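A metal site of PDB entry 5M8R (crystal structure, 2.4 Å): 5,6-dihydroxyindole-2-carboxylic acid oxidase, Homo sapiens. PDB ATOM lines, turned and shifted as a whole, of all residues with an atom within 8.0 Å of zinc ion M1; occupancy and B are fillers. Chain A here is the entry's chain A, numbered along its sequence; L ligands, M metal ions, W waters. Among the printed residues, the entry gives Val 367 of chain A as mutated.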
ATOM      1  N   HIS A 168       3.554  14.603 -21.760  1.00  0.00           N
ATOM      2  CA  HIS A 168       3.892  15.948 -21.313  1.00  0.00           C
ATOM      3  C   HIS A 168       5.399  16.188 -21.381  1.00  0.00           C
ATOM      4  O   HIS A 168       5.841  17.270 -21.802  1.00  0.00           O
ATOM      5  CB  HIS A 168       3.368  16.154 -19.876  1.00  0.00           C
ATOM      6  CG  HIS A 168       3.322  17.585 -19.421  1.00  0.00           C
ATOM      7  ND1 HIS A 168       4.289  18.147 -18.615  1.00  0.00           N
ATOM      8  CD2 HIS A 168       2.388  18.553 -19.599  1.00  0.00           C
ATOM      9  CE1 HIS A 168       3.977  19.409 -18.358  1.00  0.00           C
ATOM     10  NE2 HIS A 168       2.823  19.679 -18.935  1.00  0.00           N
ATOM     11  N   SER A 190       3.710  22.625 -25.751  1.00  0.00           N
ATOM     12  CA  SER A 190       2.498  22.630 -24.950  1.00  0.00           C
ATOM     13  C   SER A 190       2.394  23.776 -23.949  1.00  0.00           C
ATOM     14  O   SER A 190       1.389  23.850 -23.243  1.00  0.00           O
ATOM     15  CB  SER A 190       2.371  21.314 -24.183  1.00  0.00           C
ATOM     16  OG  SER A 190       3.542  21.106 -23.404  1.00  0.00           O
ATOM     17  N   HIS A 191       3.388  24.669 -23.888  1.00  0.00           N
ATOM     18  CA  HIS A 191       3.365  25.812 -22.987  1.00  0.00           C
ATOM     19  C   HIS A 191       3.905  27.021 -23.713  1.00  0.00           C
ATOM     20  O   HIS A 191       4.477  26.913 -24.796  1.00  0.00           O
ATOM     21  CB  HIS A 191       4.203  25.570 -21.719  1.00  0.00           C
ATOM     22  CG  HIS A 191       3.898  24.278 -21.059  1.00  0.00           C
ATOM     23  ND1 HIS A 191       4.301  23.058 -21.562  1.00  0.00           N
ATOM     24  CD2 HIS A 191       3.171  24.004 -19.948  1.00  0.00           C
ATOM     25  CE1 HIS A 191       3.856  22.098 -20.781  1.00  0.00           C
ATOM     26  NE2 HIS A 191       3.179  22.636 -19.791  1.00  0.00           N
ATOM     27  N   PHE A 196      -1.438  25.978 -25.302  1.00  0.00           N
ATOM     28  CA  PHE A 196      -1.314  25.551 -23.910  1.00  0.00           C
ATOM     29  C   PHE A 196      -2.623  24.942 -23.392  1.00  0.00           C
ATOM     30  O   PHE A 196      -2.628  23.860 -22.793  1.00  0.00           O
ATOM     31  CB  PHE A 196      -0.890  26.738 -23.033  1.00  0.00           C
ATOM     32  CG  PHE A 196      -1.137  26.517 -21.555  1.00  0.00           C
ATOM     33  CD1 PHE A 196      -0.313  25.689 -20.808  1.00  0.00           C
ATOM     34  CD2 PHE A 196      -2.211  27.139 -20.919  1.00  0.00           C
ATOM     35  CE1 PHE A 196      -0.562  25.471 -19.453  1.00  0.00           C
ATOM     36  CE2 PHE A 196      -2.454  26.925 -19.576  1.00  0.00           C
ATOM     37  CZ  PHE A 196      -1.633  26.101 -18.838  1.00  0.00           C
ATOM     38  N   HIS A 200      -3.440  20.802 -23.043  1.00  0.00           N
ATOM     39  CA  HIS A 200      -3.697  20.204 -21.727  1.00  0.00           C
ATOM     40  C   HIS A 200      -5.116  19.685 -21.623  1.00  0.00           C
ATOM     41  O   HIS A 200      -5.358  18.747 -20.864  1.00  0.00           O
ATOM     42  CB  HIS A 200      -3.391  21.203 -20.608  1.00  0.00           C
ATOM     43  CG  HIS A 200      -1.920  21.384 -20.367  1.00  0.00           C
ATOM     44  ND1 HIS A 200      -1.124  22.168 -21.168  1.00  0.00           N
ATOM     45  CD2 HIS A 200      -1.087  20.822 -19.446  1.00  0.00           C
ATOM     46  CE1 HIS A 200       0.125  22.109 -20.747  1.00  0.00           C
ATOM     47  NE2 HIS A 200       0.174  21.313 -19.695  1.00  0.00           N
ATOM     48  N   HIS A 203      -4.904  16.200 -23.189  1.00  0.00           N
ATOM     49  CA  HIS A 203      -4.150  15.473 -22.180  1.00  0.00           C
ATOM     50  C   HIS A 203      -5.066  14.905 -21.096  1.00  0.00           C
ATOM     51  O   HIS A 203      -5.054  13.695 -20.818  1.00  0.00           O
ATOM     52  CB  HIS A 203      -3.123  16.438 -21.576  1.00  0.00           C
ATOM     53  CG  HIS A 203      -2.016  15.783 -20.818  1.00  0.00           C
ATOM     54  ND1 HIS A 203      -1.424  16.378 -19.721  1.00  0.00           N
ATOM     55  CD2 HIS A 203      -1.348  14.618 -21.021  1.00  0.00           C
ATOM     56  CE1 HIS A 203      -0.470  15.591 -19.258  1.00  0.00           C
ATOM     57  NE2 HIS A 203      -0.395  14.524 -20.033  1.00  0.00           N
ATOM     58  N   GLU A 336      -2.672  30.921 -18.085  1.00  0.00           N
ATOM     59  CA  GLU A 336      -1.454  30.138 -17.983  1.00  0.00           C
ATOM     60  C   GLU A 336      -0.574  30.665 -16.862  1.00  0.00           C
ATOM     61  O   GLU A 336       0.040  29.884 -16.131  1.00  0.00           O
ATOM     62  CB  GLU A 336      -0.686  30.115 -19.311  1.00  0.00           C
ATOM     63  CG  GLU A 336       0.557  29.222 -19.183  1.00  0.00           C
ATOM     64  CD  GLU A 336       1.318  28.991 -20.468  1.00  0.00           C
ATOM     65  OE1 GLU A 336       0.909  29.519 -21.517  1.00  0.00           O
ATOM     66  OE2 GLU A 336       2.337  28.253 -20.410  1.00  0.00           O
ATOM     67  N   HIS A 353      -2.350  29.498 -13.057  1.00  0.00           N
ATOM     68  CA  HIS A 353      -1.877  28.116 -13.263  1.00  0.00           C
ATOM     69  C   HIS A 353      -0.389  27.961 -12.959  1.00  0.00           C
ATOM     70  O   HIS A 353       0.024  26.982 -12.337  1.00  0.00           O
ATOM     71  CB  HIS A 353      -2.192  27.676 -14.698  1.00  0.00           C
ATOM     72  CG  HIS A 353      -1.233  26.670 -15.254  1.00  0.00           C
ATOM     73  ND1 HIS A 353      -0.110  27.026 -15.965  1.00  0.00           N
ATOM     74  CD2 HIS A 353      -1.228  25.317 -15.192  1.00  0.00           C
ATOM     75  CE1 HIS A 353       0.550  25.943 -16.326  1.00  0.00           C
ATOM     76  NE2 HIS A 353      -0.114  24.879 -15.871  1.00  0.00           N
ATOM     77  N   ASN A 354       0.441  28.911 -13.408  1.00  0.00           N
ATOM     78  CA  ASN A 354       1.860  28.847 -13.075  1.00  0.00           C
ATOM     79  C   ASN A 354       2.071  28.913 -11.560  1.00  0.00           C
ATOM     80  O   ASN A 354       2.886  28.159 -11.008  1.00  0.00           O
ATOM     81  CB  ASN A 354       2.617  29.980 -13.766  1.00  0.00           C
ATOM     82  CG  ASN A 354       2.854  29.728 -15.239  1.00  0.00           C
ATOM     83  OD1 ASN A 354       2.795  28.594 -15.716  1.00  0.00           O
ATOM     84  ND2 ASN A 354       3.175  30.777 -15.971  1.00  0.00           N
ATOM     85  N   ALA A 356       0.038  28.076  -9.056  1.00  0.00           N
ATOM     86  CA  ALA A 356      -0.319  26.831  -8.391  1.00  0.00           C
ATOM     87  C   ALA A 356       0.803  25.802  -8.525  1.00  0.00           C
ATOM     88  O   ALA A 356       1.066  25.039  -7.586  1.00  0.00           O
ATOM     89  CB  ALA A 356      -1.641  26.300  -8.936  1.00  0.00           C
ATOM     90  N   HIS A 357       1.488  25.783  -9.672  1.00  0.00           N
ATOM     91  CA  HIS A 357       2.593  24.844  -9.843  1.00  0.00           C
ATOM     92  C   HIS A 357       3.735  25.168  -8.903  1.00  0.00           C
ATOM     93  O   HIS A 357       4.287  24.279  -8.240  1.00  0.00           O
ATOM     94  CB  HIS A 357       3.120  24.881 -11.273  1.00  0.00           C
ATOM     95  CG  HIS A 357       2.422  23.975 -12.229  1.00  0.00           C
ATOM     96  ND1 HIS A 357       2.647  22.607 -12.267  1.00  0.00           N
ATOM     97  CD2 HIS A 357       1.534  24.226 -13.222  1.00  0.00           C
ATOM     98  CE1 HIS A 357       1.919  22.072 -13.232  1.00  0.00           C
ATOM     99  NE2 HIS A 357       1.242  23.030 -13.820  1.00  0.00           N
ATOM    100  N   GLY A 364       5.969  18.857  -8.692  1.00  0.00           N
ATOM    101  CA  GLY A 364       4.910  19.544  -9.431  1.00  0.00           C
ATOM    102  C   GLY A 364       5.266  20.932  -9.934  1.00  0.00           C
ATOM    103  O   GLY A 364       4.492  21.513 -10.721  1.00  0.00           O
ATOM    104  N   VAL A 367       8.457  21.702 -15.087  1.00  0.00           N
ATOM    105  CA  VAL A 367       7.541  21.459 -16.215  1.00  0.00           C
ATOM    106  C   VAL A 367       7.790  20.095 -16.868  1.00  0.00           C
ATOM    107  O   VAL A 367       6.845  19.453 -17.325  1.00  0.00           O
ATOM    108  CB  VAL A 367       7.621  22.632 -17.217  1.00  0.00           C
ATOM    109  CG1 VAL A 367       8.914  22.644 -17.939  1.00  0.00           C
ATOM    110  CG2 VAL A 367       6.448  22.598 -18.209  1.00  0.00           C
ATOM    111  N   SER A 370       6.195  17.657 -13.834  1.00  0.00           N
ATOM    112  CA  SER A 370       5.117  17.981 -12.919  1.00  0.00           C
ATOM    113  C   SER A 370       3.921  17.013 -12.957  1.00  0.00           C
ATOM    114  O   SER A 370       3.322  16.829 -11.892  1.00  0.00           O
ATOM    115  CB  SER A 370       4.706  19.436 -13.152  1.00  0.00           C
ATOM    116  OG  SER A 370       4.264  19.652 -14.476  1.00  0.00           O
ATOM    117  N   PRO A 371       3.585  16.323 -14.064  1.00  0.00           N
ATOM    118  CA  PRO A 371       2.495  15.323 -13.960  1.00  0.00           C
ATOM    119  C   PRO A 371       2.808  14.178 -13.014  1.00  0.00           C
ATOM    120  O   PRO A 371       1.868  13.459 -12.636  1.00  0.00           O
ATOM    121  CB  PRO A 371       2.331  14.795 -15.397  1.00  0.00           C
ATOM    122  CG  PRO A 371       2.970  15.818 -16.282  1.00  0.00           C
ATOM    123  CD  PRO A 371       4.071  16.424 -15.453  1.00  0.00           C
ATOM    124  N   PHE A 376      -1.308  17.462 -10.350  1.00  0.00           N
ATOM    125  CA  PHE A 376      -1.327  17.993 -11.704  1.00  0.00           C
ATOM    126  C   PHE A 376      -2.703  17.809 -12.360  1.00  0.00           C
ATOM    127  O   PHE A 376      -3.245  18.749 -12.961  1.00  0.00           O
ATOM    128  CB  PHE A 376      -0.225  17.292 -12.508  1.00  0.00           C
ATOM    129  CG  PHE A 376      -0.114  17.749 -13.953  1.00  0.00           C
ATOM    130  CD1 PHE A 376      -0.960  17.246 -14.917  1.00  0.00           C
ATOM    131  CD2 PHE A 376       0.862  18.656 -14.326  1.00  0.00           C
ATOM    132  CE1 PHE A 376      -0.855  17.635 -16.239  1.00  0.00           C
ATOM    133  CE2 PHE A 376       0.981  19.052 -15.639  1.00  0.00           C
ATOM    134  CZ  PHE A 376       0.112  18.542 -16.608  1.00  0.00           C
ATOM    135  N   LEU A 379      -5.161  20.218 -10.689  1.00  0.00           N
ATOM    136  CA  LEU A 379      -4.750  21.568 -11.045  1.00  0.00           C
ATOM    137  C   LEU A 379      -5.133  21.909 -12.489  1.00  0.00           C
ATOM    138  O   LEU A 379      -5.533  23.045 -12.789  1.00  0.00           O
ATOM    139  CB  LEU A 379      -3.230  21.688 -10.824  1.00  0.00           C
ATOM    140  CG  LEU A 379      -2.437  22.981 -10.981  1.00  0.00           C
ATOM    141  CD1 LEU A 379      -1.029  22.722 -10.438  1.00  0.00           C
ATOM    142  CD2 LEU A 379      -2.340  23.422 -12.438  1.00  0.00           C
ATOM    143  N   HIS A 380      -5.035  20.933 -13.396  1.00  0.00           N
ATOM    144  CA  HIS A 380      -5.378  21.190 -14.797  1.00  0.00           C
ATOM    145  C   HIS A 380      -6.845  20.974 -15.147  1.00  0.00           C
ATOM    146  O   HIS A 380      -7.336  21.638 -16.052  1.00  0.00           O
ATOM    147  CB  HIS A 380      -4.509  20.346 -15.733  1.00  0.00           C
ATOM    148  CG  HIS A 380      -3.304  21.095 -16.200  1.00  0.00           C
ATOM    149  ND1 HIS A 380      -3.373  22.106 -17.133  1.00  0.00           N
ATOM    150  CD2 HIS A 380      -2.021  21.062 -15.769  1.00  0.00           C
ATOM    151  CE1 HIS A 380      -2.184  22.641 -17.281  1.00  0.00           C
ATOM    152  NE2 HIS A 380      -1.339  22.016 -16.481  1.00  0.00           N
ATOM    153  N   THR A 383      -7.917  24.442 -14.409  1.00  0.00           N
ATOM    154  CA  THR A 383      -7.540  25.322 -15.506  1.00  0.00           C
ATOM    155  C   THR A 383      -8.414  25.089 -16.726  1.00  0.00           C
ATOM    156  O   THR A 383      -8.774  26.033 -17.440  1.00  0.00           O
ATOM    157  CB  THR A 383      -6.071  25.103 -15.885  1.00  0.00           C
ATOM    158  OG1 THR A 383      -5.226  25.244 -14.726  1.00  0.00           O
ATOM    159  CG2 THR A 383      -5.659  26.101 -16.959  1.00  0.00           C
HETATM  160  O1  LIG L   1       3.113  24.363 -16.747  1.00  0.00           O
HETATM  161  C1  LIG L   1       6.928  29.419 -14.678  1.00  0.00           C
HETATM  162  O2  LIG L   1       6.211  30.105 -13.899  1.00  0.00           O
HETATM  163  O3  LIG L   1       8.081  29.821 -15.004  1.00  0.00           O
HETATM  164  N1  LIG L   1       7.480  27.414 -15.982  1.00  0.00           N
HETATM  165  C2  LIG L   1       6.422  28.090 -15.238  1.00  0.00           C
HETATM  166  C3  LIG L   1       5.991  27.254 -14.046  1.00  0.00           C
HETATM  167  N2  LIG L   1       5.523  25.942 -14.408  1.00  0.00           N
HETATM  168  C4  LIG L   1       4.493  25.779 -15.461  1.00  0.00           C
HETATM  169  C5  LIG L   1       6.073  24.746 -13.698  1.00  0.00           C
HETATM  170  C6  LIG L   1       4.082  24.561 -15.771  1.00  0.00           C
HETATM  171  C7  LIG L   1       5.653  23.528 -14.005  1.00  0.00           C
HETATM  172  C8  LIG L   1       4.608  23.349 -15.070  1.00  0.00           C
HETATM  173  O4  LIG L   1       4.193  22.279 -15.375  1.00  0.00           O
HETATM  174 ZN    ZN M   1       0.492  22.892 -15.780  1.00  0.00          ZN
HETATM  175 ZN    ZN M   2       1.907  21.445 -18.702  1.00  0.00          ZN
HETATM  176  O   HOH W   1       2.073  22.119 -16.738  1.00  0.00           O
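A ring nitrogen (ND1) of His 357 sits close to an oxygen (O4) of the ligand (3.5 Å). The side-chain hydroxyl of Ser 370 lies within hydrogen-bond range of an oxygen (O4) of the ligand, at 2.8 Å. O1 of the ligand lies close to NE2 of His 353, 3.4 Å away. A ring nitrogen (NE2) of His 191 sits close to an oxygen (O1) of the ligand.
Water W1 binds zinc ion M1, at 2.0 Å. A ring nitrogen (NE2) of His 353 binds zinc ion M1. NE2 of His 357 is bound to zinc ion M1. A ring nitrogen (NE2) of His 380 binds zinc ion M1 (2.1 Å). Zinc ion M1 has four donor atoms within binding distance.
O of Glu 336 lies within hydrogen-bond range of ND1 of His 353, at 2.9 Å. A ring nitrogen (ND1) of His 357 is in hydrogen-bond range of the backbone carbonyl oxygen (O) of Gly 364 (2.6 Å). A ring nitrogen (ND1) of His 353 is in hydrogen-bond range of the side-chain amide oxygen (OD1) of Asn 354 (3.3 Å).
Residues that only touch zinc ion M1: Phe 376 (3.9 Å). Within 4 Å of zinc ion M1: His 353, His 357, Phe 376 and His 380. The nearest printed residue that does not touch zinc ion M1 is His 200 (4.2 Å).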
